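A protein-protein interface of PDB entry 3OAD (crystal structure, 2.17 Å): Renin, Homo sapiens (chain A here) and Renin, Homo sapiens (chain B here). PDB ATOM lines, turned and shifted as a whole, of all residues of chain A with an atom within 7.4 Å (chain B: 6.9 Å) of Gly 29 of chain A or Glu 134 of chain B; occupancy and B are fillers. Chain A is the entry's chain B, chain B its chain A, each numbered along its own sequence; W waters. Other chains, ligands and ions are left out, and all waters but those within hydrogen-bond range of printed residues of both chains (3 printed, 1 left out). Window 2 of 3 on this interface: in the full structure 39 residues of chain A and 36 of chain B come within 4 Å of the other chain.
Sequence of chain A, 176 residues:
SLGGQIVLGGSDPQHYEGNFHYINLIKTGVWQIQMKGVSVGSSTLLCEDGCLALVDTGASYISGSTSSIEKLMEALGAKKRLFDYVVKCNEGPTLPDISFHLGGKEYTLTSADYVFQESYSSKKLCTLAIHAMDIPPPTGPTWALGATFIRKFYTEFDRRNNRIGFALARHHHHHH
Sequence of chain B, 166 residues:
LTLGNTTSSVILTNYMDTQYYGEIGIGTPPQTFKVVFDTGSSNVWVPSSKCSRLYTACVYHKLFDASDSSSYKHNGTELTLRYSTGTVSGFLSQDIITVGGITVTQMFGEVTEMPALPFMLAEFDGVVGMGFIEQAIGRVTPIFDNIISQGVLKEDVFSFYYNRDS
The side-chain amide oxygen (OE1) of Gln 135 of chain B lies within hydrogen-bond range of the side-chain hydroxyl (OG1) of Thr 139 of chain A (3.3 Å). The side-chain carboxylate (OD1) of Asp 145 of chain B lies within salt-bridge range of the guanidinium group (NH1) of Arg 159 of chain A.
Of chain A, only Gly 29 comes within 4 Å of Glu 134 of chain B. Of the printed residues of chain A, Asp 145 of chain B touches Arg 159 (3.1 Å). Of the printed residues of chain B, Trp 31 of chain A touches Gly 131 and Phe 132. Of the printed residues of chain A, Phe 132 of chain B touches Leu 25 (3.7 Å), Thr 28 (3.2 Å), Gly 29 (3.1 Å), Val 30 (3.6 Å), Trp 31 (3.4 Å), Arg 159 (3.4 Å) and Asn 162 (3.8 Å). The nearest residue of chain A that does not touch Glu 134 of chain B is Thr 28 of chain A (4.2 Å).
Among the printed residues, merely in contact across the chains: Gly 29 of chain A with Phe 132 of chain B (3.1 Å), Gly 29 of chain A with Gln 135 of chain B (3.2 Å), Thr 28 of chain A with Phe 132 of chain B (3.2 Å), Trp 31 of chain A with Phe 132 of chain B (3.4 Å), Arg 159 of chain A with Phe 132 of chain B (3.4 Å), Val 30 of chain A with Phe 132 of chain B (3.6 Å), Trp 31 of chain A with Gly 131 of chain B (3.6 Å), Leu 25 of chain A with Phe 132 of chain B (3.7 Å), Gly 29 of chain A with Glu 134 of chain B (3.8 Å) and Asn 162 of chain A with Phe 132 of chain B (3.8 Å).
OG of Ser 42 of chain B sits at hydrogen-bond distance from O of Phe 132 of chain B, at 2.7 Å. The backbone NH (N) of Leu 25 of chain A sits at hydrogen-bond distance from the backbone carbonyl oxygen (O) of Asn 162 of chain A. OG1 of Thr 28 of chain A is in hydrogen-bond range of OD1 of Asn 162 of chain A, 3.2 Å away. OE1 of Gln 32 of chain A sits close to O of Thr 139 of chain A (2.9 Å).
Water W3 lies within hydrogen-bond range of the side-chain carboxylate of Asp 145 of chain B (2.5 Å), the backbone NH of Ile 133 of chain B (2.8 Å) and the guanidinium group of Arg 159 of chain A (3.3 Å). Water W1 lies within hydrogen-bond range of the backbone NH of Phe 132 of chain B (2.7 Å), the backbone carbonyl oxygen of Gly 29 of chain A (3.0 Å) and the side-chain hydroxyl of Ser 42 of chain B (3.3 Å). Water W2 bridges NH1 of Arg 159 of chain A (3.1 Å) and O of Gly 131 of chain B (3.5 Å).
Of the 11 printed residues of chain B, 5 touch a printed residue of chain A. Printed residues of chain B that touch a printed residue of chain A: Gly 131, Phe 132, Glu 134, Gln 135 and Asp 145. Of the 11 printed residues of chain A, 8 touch a printed residue of chain B. Hydrophobic or aromatic side chains of chain A within 4 Å of the printed part of chain B: Leu 25 and Trp 31. Along chain A the printed residues that touch a printed residue of chain B span positions 25 to 162. Among the printed residues, 12 pairs touch across the chains.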
ATOM      1  N   LEU A  25       6.370 -12.638  -6.390  1.00  0.00           N
ATOM      2  CA  LEU A  25       7.010 -13.761  -7.039  1.00  0.00           C
ATOM      3  C   LEU A  25       6.410 -13.867  -8.440  1.00  0.00           C
ATOM      4  O   LEU A  25       5.255 -13.465  -8.662  1.00  0.00           O
ATOM      5  CB  LEU A  25       6.817 -15.073  -6.255  1.00  0.00           C
ATOM      6  CG  LEU A  25       7.035 -15.264  -4.735  1.00  0.00           C
ATOM      7  CD1 LEU A  25       7.142 -16.759  -4.454  1.00  0.00           C
ATOM      8  CD2 LEU A  25       8.250 -14.558  -4.178  1.00  0.00           C
ATOM      9  N   LYS A  27       5.978 -16.826 -10.064  1.00  0.00           N
ATOM     10  CA  LYS A  27       5.013 -17.885  -9.791  1.00  0.00           C
ATOM     11  C   LYS A  27       5.209 -18.365  -8.361  1.00  0.00           C
ATOM     12  O   LYS A  27       6.335 -18.359  -7.848  1.00  0.00           O
ATOM     13  CB  LYS A  27       5.159 -19.061 -10.762  1.00  0.00           C
ATOM     14  CG  LYS A  27       6.586 -19.603 -10.914  1.00  0.00           C
ATOM     15  CD  LYS A  27       6.600 -21.066 -11.353  1.00  0.00           C
ATOM     16  CE  LYS A  27       7.660 -21.319 -12.440  1.00  0.00           C
ATOM     17  NZ  LYS A  27       9.032 -20.801 -12.117  1.00  0.00           N
ATOM     18  N   THR A  28       4.102 -18.738  -7.713  1.00  0.00           N
ATOM     19  CA  THR A  28       4.144 -19.506  -6.487  1.00  0.00           C
ATOM     20  C   THR A  28       4.756 -20.825  -6.911  1.00  0.00           C
ATOM     21  O   THR A  28       4.625 -21.219  -8.076  1.00  0.00           O
ATOM     22  CB  THR A  28       2.725 -19.667  -5.842  1.00  0.00           C
ATOM     23  OG1 THR A  28       2.853 -20.061  -4.465  1.00  0.00           O
ATOM     24  CG2 THR A  28       1.830 -20.664  -6.606  1.00  0.00           C
ATOM     25  N   GLY A  29       5.462 -21.479  -6.000  1.00  0.00           N
ATOM     26  CA  GLY A  29       6.236 -22.663  -6.359  1.00  0.00           C
ATOM     27  C   GLY A  29       7.707 -22.527  -6.036  1.00  0.00           C
ATOM     28  O   GLY A  29       8.318 -23.467  -5.559  1.00  0.00           O
ATOM     29  N   VAL A  30       8.270 -21.350  -6.287  1.00  0.00           N
ATOM     30  CA  VAL A  30       9.700 -21.102  -6.129  1.00  0.00           C
ATOM     31  C   VAL A  30       9.907 -19.705  -5.575  1.00  0.00           C
ATOM     32  O   VAL A  30       9.205 -18.772  -5.993  1.00  0.00           O
ATOM     33  CB  VAL A  30      10.437 -21.263  -7.493  1.00  0.00           C
ATOM     34  CG1 VAL A  30       9.941 -20.267  -8.506  1.00  0.00           C
ATOM     35  CG2 VAL A  30      11.963 -21.144  -7.347  1.00  0.00           C
ATOM     36  N   TRP A  31      10.853 -19.548  -4.645  1.00  0.00           N
ATOM     37  CA  TRP A  31      11.210 -18.229  -4.121  1.00  0.00           C
ATOM     38  C   TRP A  31      12.062 -17.418  -5.098  1.00  0.00           C
ATOM     39  O   TRP A  31      13.206 -17.069  -4.804  1.00  0.00           O
ATOM     40  CB  TRP A  31      11.906 -18.325  -2.767  1.00  0.00           C
ATOM     41  CG  TRP A  31      11.004 -18.699  -1.645  1.00  0.00           C
ATOM     42  CD1 TRP A  31      11.009 -19.869  -0.962  1.00  0.00           C
ATOM     43  CD2 TRP A  31       9.960 -17.905  -1.075  1.00  0.00           C
ATOM     44  NE1 TRP A  31      10.035 -19.863   0.000  1.00  0.00           N
ATOM     45  CE2 TRP A  31       9.376 -18.665  -0.042  1.00  0.00           C
ATOM     46  CE3 TRP A  31       9.462 -16.625  -1.331  1.00  0.00           C
ATOM     47  CZ2 TRP A  31       8.313 -18.192   0.734  1.00  0.00           C
ATOM     48  CZ3 TRP A  31       8.397 -16.151  -0.552  1.00  0.00           C
ATOM     49  CH2 TRP A  31       7.840 -16.939   0.464  1.00  0.00           C
ATOM     50  N   GLN A  32      11.461 -17.092  -6.244  1.00  0.00           N
ATOM     51  CA  GLN A  32      12.118 -16.410  -7.346  1.00  0.00           C
ATOM     52  C   GLN A  32      11.357 -15.157  -7.795  1.00  0.00           C
ATOM     53  O   GLN A  32      10.140 -15.181  -7.971  1.00  0.00           O
ATOM     54  CB  GLN A  32      12.219 -17.383  -8.524  1.00  0.00           C
ATOM     55  CG  GLN A  32      13.317 -17.100  -9.527  1.00  0.00           C
ATOM     56  CD  GLN A  32      13.407 -18.204 -10.581  1.00  0.00           C
ATOM     57  OE1 GLN A  32      14.487 -18.483 -11.107  1.00  0.00           O
ATOM     58  NE2 GLN A  32      12.271 -18.844 -10.887  1.00  0.00           N
ATOM     59  N   PRO A 138      13.533 -26.676 -13.946  1.00  0.00           N
ATOM     60  CA  PRO A 138      12.644 -25.510 -14.107  1.00  0.00           C
ATOM     61  C   PRO A 138      13.231 -24.174 -13.636  1.00  0.00           C
ATOM     62  O   PRO A 138      13.227 -23.207 -14.403  1.00  0.00           O
ATOM     63  CB  PRO A 138      11.407 -25.885 -13.272  1.00  0.00           C
ATOM     64  CG  PRO A 138      11.733 -27.217 -12.583  1.00  0.00           C
ATOM     65  CD  PRO A 138      13.196 -27.459 -12.740  1.00  0.00           C
ATOM     66  N   THR A 139      13.737 -24.144 -12.399  1.00  0.00           N
ATOM     67  CA  THR A 139      14.221 -22.927 -11.729  1.00  0.00           C
ATOM     68  C   THR A 139      15.126 -22.063 -12.615  1.00  0.00           C
ATOM     69  O   THR A 139      14.896 -20.858 -12.753  1.00  0.00           O
ATOM     70  CB  THR A 139      14.998 -23.288 -10.435  1.00  0.00           C
ATOM     71  OG1 THR A 139      14.162 -24.051  -9.558  1.00  0.00           O
ATOM     72  CG2 THR A 139      15.481 -22.051  -9.716  1.00  0.00           C
ATOM     73  N   ARG A 159       4.472 -15.757   2.636  1.00  0.00           N
ATOM     74  CA  ARG A 159       3.624 -16.763   1.996  1.00  0.00           C
ATOM     75  C   ARG A 159       2.161 -16.342   1.716  1.00  0.00           C
ATOM     76  O   ARG A 159       1.600 -16.652   0.641  1.00  0.00           O
ATOM     77  CB  ARG A 159       3.702 -18.091   2.757  1.00  0.00           C
ATOM     78  CG  ARG A 159       4.998 -18.878   2.489  1.00  0.00           C
ATOM     79  CD  ARG A 159       5.046 -19.480   1.096  1.00  0.00           C
ATOM     80  NE  ARG A 159       3.917 -20.377   0.888  1.00  0.00           N
ATOM     81  CZ  ARG A 159       3.889 -21.670   1.189  1.00  0.00           C
ATOM     82  NH1 ARG A 159       4.943 -22.274   1.700  1.00  0.00           N
ATOM     83  NH2 ARG A 159       2.785 -22.370   0.974  1.00  0.00           N
ATOM     84  N   ASN A 162       2.693 -14.041  -1.267  1.00  0.00           N
ATOM     85  CA  ASN A 162       3.628 -14.535  -2.279  1.00  0.00           C
ATOM     86  C   ASN A 162       4.535 -13.433  -2.760  1.00  0.00           C
ATOM     87  O   ASN A 162       4.612 -13.125  -3.976  1.00  0.00           O
ATOM     88  CB  ASN A 162       2.897 -15.137  -3.475  1.00  0.00           C
ATOM     89  CG  ASN A 162       2.332 -16.494  -3.184  1.00  0.00           C
ATOM     90  OD1 ASN A 162       3.042 -17.414  -2.744  1.00  0.00           O
ATOM     91  ND2 ASN A 162       1.043 -16.642  -3.446  1.00  0.00           N
ATOM     92  N   SER B  42      13.203 -27.476  -0.320  1.00  0.00           N
ATOM     93  CA  SER B  42      11.865 -27.669   0.275  1.00  0.00           C
ATOM     94  C   SER B  42      11.744 -28.873   1.202  1.00  0.00           C
ATOM     95  O   SER B  42      10.692 -29.065   1.798  1.00  0.00           O
ATOM     96  CB  SER B  42      10.805 -27.826  -0.812  1.00  0.00           C
ATOM     97  OG  SER B  42      10.660 -26.652  -1.589  1.00  0.00           O
ATOM     98  N   GLY B 131      11.317 -23.724   1.146  1.00  0.00           N
ATOM     99  CA  GLY B 131      10.614 -23.448  -0.101  1.00  0.00           C
ATOM    100  C   GLY B 131       9.285 -24.176  -0.123  1.00  0.00           C
ATOM    101  O   GLY B 131       8.809 -24.643   0.924  1.00  0.00           O
ATOM    102  N   PHE B 132       8.736 -24.298  -1.338  1.00  0.00           N
ATOM    103  CA  PHE B 132       7.345 -24.668  -1.634  1.00  0.00           C
ATOM    104  C   PHE B 132       7.191 -26.152  -1.928  1.00  0.00           C
ATOM    105  O   PHE B 132       8.106 -26.785  -2.471  1.00  0.00           O
ATOM    106  CB  PHE B 132       6.832 -23.907  -2.879  1.00  0.00           C
ATOM    107  CG  PHE B 132       6.648 -22.410  -2.677  1.00  0.00           C
ATOM    108  CD1 PHE B 132       7.738 -21.536  -2.713  1.00  0.00           C
ATOM    109  CD2 PHE B 132       5.383 -21.877  -2.474  1.00  0.00           C
ATOM    110  CE1 PHE B 132       7.571 -20.169  -2.534  1.00  0.00           C
ATOM    111  CE2 PHE B 132       5.218 -20.512  -2.287  1.00  0.00           C
ATOM    112  CZ  PHE B 132       6.315 -19.656  -2.309  1.00  0.00           C
ATOM    113  N   ILE B 133       6.011 -26.692  -1.619  1.00  0.00           N
ATOM    114  CA  ILE B 133       5.708 -28.101  -1.916  1.00  0.00           C
ATOM    115  C   ILE B 133       6.016 -28.500  -3.372  1.00  0.00           C
ATOM    116  O   ILE B 133       6.373 -29.641  -3.626  1.00  0.00           O
ATOM    117  CB  ILE B 133       4.254 -28.498  -1.502  1.00  0.00           C
ATOM    118  CG1 ILE B 133       4.127 -30.018  -1.407  1.00  0.00           C
ATOM    119  CG2 ILE B 133       3.227 -27.905  -2.461  1.00  0.00           C
ATOM    120  CD1 ILE B 133       3.224 -30.508  -0.301  1.00  0.00           C
ATOM    121  N   GLU B 134       5.931 -27.549  -4.307  1.00  0.00           N
ATOM    122  CA  GLU B 134       6.226 -27.817  -5.718  1.00  0.00           C
ATOM    123  C   GLU B 134       7.640 -28.292  -5.924  1.00  0.00           C
ATOM    124  O   GLU B 134       7.898 -29.123  -6.779  1.00  0.00           O
ATOM    125  CB  GLU B 134       5.985 -26.581  -6.588  1.00  0.00           C
ATOM    126  CG  GLU B 134       4.542 -26.369  -6.954  1.00  0.00           C
ATOM    127  CD  GLU B 134       3.786 -25.482  -5.984  1.00  0.00           C
ATOM    128  OE1 GLU B 134       4.017 -25.530  -4.750  1.00  0.00           O
ATOM    129  OE2 GLU B 134       2.948 -24.716  -6.484  1.00  0.00           O
ATOM    130  N   GLN B 135       8.560 -27.765  -5.126  1.00  0.00           N
ATOM    131  CA  GLN B 135       9.971 -28.085  -5.288  1.00  0.00           C
ATOM    132  C   GLN B 135      10.433 -29.221  -4.376  1.00  0.00           C
ATOM    133  O   GLN B 135      11.604 -29.606  -4.413  1.00  0.00           O
ATOM    134  CB  GLN B 135      10.809 -26.834  -5.074  1.00  0.00           C
ATOM    135  CG  GLN B 135      10.552 -25.747  -6.118  1.00  0.00           C
ATOM    136  CD  GLN B 135      11.623 -25.706  -7.183  1.00  0.00           C
ATOM    137  OE1 GLN B 135      12.805 -25.527  -6.877  1.00  0.00           O
ATOM    138  NE2 GLN B 135      11.221 -25.859  -8.446  1.00  0.00           N
ATOM    139  N   ALA B 136       9.500 -29.749  -3.576  1.00  0.00           N
ATOM    140  CA  ALA B 136       9.767 -30.827  -2.641  1.00  0.00           C
ATOM    141  C   ALA B 136       9.917 -32.161  -3.339  1.00  0.00           C
ATOM    142  O   ALA B 136       9.090 -32.568  -4.169  1.00  0.00           O
ATOM    143  CB  ALA B 136       8.672 -30.911  -1.582  1.00  0.00           C
ATOM    144  N   ILE B 137      10.975 -32.856  -2.970  1.00  0.00           N
ATOM    145  CA  ILE B 137      11.247 -34.165  -3.519  1.00  0.00           C
ATOM    146  C   ILE B 137      10.270 -35.158  -2.911  1.00  0.00           C
ATOM    147  O   ILE B 137      10.121 -35.222  -1.686  1.00  0.00           O
ATOM    148  CB  ILE B 137      12.708 -34.557  -3.261  1.00  0.00           C
ATOM    149  CG1 ILE B 137      13.633 -33.519  -3.934  1.00  0.00           C
ATOM    150  CG2 ILE B 137      12.961 -35.992  -3.705  1.00  0.00           C
ATOM    151  CD1 ILE B 137      15.110 -33.752  -3.726  1.00  0.00           C
ATOM    152  N   ARG B 139       7.198 -34.771  -3.209  1.00  0.00           N
ATOM    153  CA  ARG B 139       6.064 -33.925  -2.831  1.00  0.00           C
ATOM    154  C   ARG B 139       5.723 -34.060  -1.322  1.00  0.00           C
ATOM    155  O   ARG B 139       4.547 -34.043  -0.920  1.00  0.00           O
ATOM    156  CB  ARG B 139       4.865 -34.225  -3.756  1.00  0.00           C
ATOM    157  CG  ARG B 139       3.782 -33.149  -3.784  1.00  0.00           C
ATOM    158  CD  ARG B 139       2.896 -33.219  -5.039  1.00  0.00           C
ATOM    159  NE  ARG B 139       2.110 -31.986  -5.232  1.00  0.00           N
ATOM    160  CZ  ARG B 139       2.570 -30.873  -5.811  1.00  0.00           C
ATOM    161  NH1 ARG B 139       3.825 -30.808  -6.245  1.00  0.00           N
ATOM    162  NH2 ARG B 139       1.778 -29.811  -5.941  1.00  0.00           N
ATOM    163  N   PRO B 142       6.452 -29.597   3.197  1.00  0.00           N
ATOM    164  CA  PRO B 142       7.548 -28.871   3.844  1.00  0.00           C
ATOM    165  C   PRO B 142       7.169 -28.335   5.211  1.00  0.00           C
ATOM    166  O   PRO B 142       5.982 -28.099   5.482  1.00  0.00           O
ATOM    167  CB  PRO B 142       7.836 -27.715   2.870  1.00  0.00           C
ATOM    168  CG  PRO B 142       7.155 -28.122   1.573  1.00  0.00           C
ATOM    169  CD  PRO B 142       5.942 -28.865   2.023  1.00  0.00           C
ATOM    170  N   ASP B 145       4.947 -25.262   5.682  1.00  0.00           N
ATOM    171  CA  ASP B 145       3.556 -25.609   5.386  1.00  0.00           C
ATOM    172  C   ASP B 145       2.864 -26.180   6.623  1.00  0.00           C
ATOM    173  O   ASP B 145       1.766 -25.751   6.978  1.00  0.00           O
ATOM    174  CB  ASP B 145       3.468 -26.555   4.208  1.00  0.00           C
ATOM    175  CG  ASP B 145       3.771 -25.865   2.911  1.00  0.00           C
ATOM    176  OD1 ASP B 145       4.791 -25.138   2.837  1.00  0.00           O
ATOM    177  OD2 ASP B 145       2.975 -26.048   1.957  1.00  0.00           O
HETATM  178  O   HOH W   1      10.350 -23.899  -3.423  1.00  0.00           O
HETATM  179  O   HOH W   2       7.898 -21.678   2.484  1.00  0.00           O
HETATM  180  O   HOH W   3       4.282 -25.192  -0.024  1.00  0.00           O
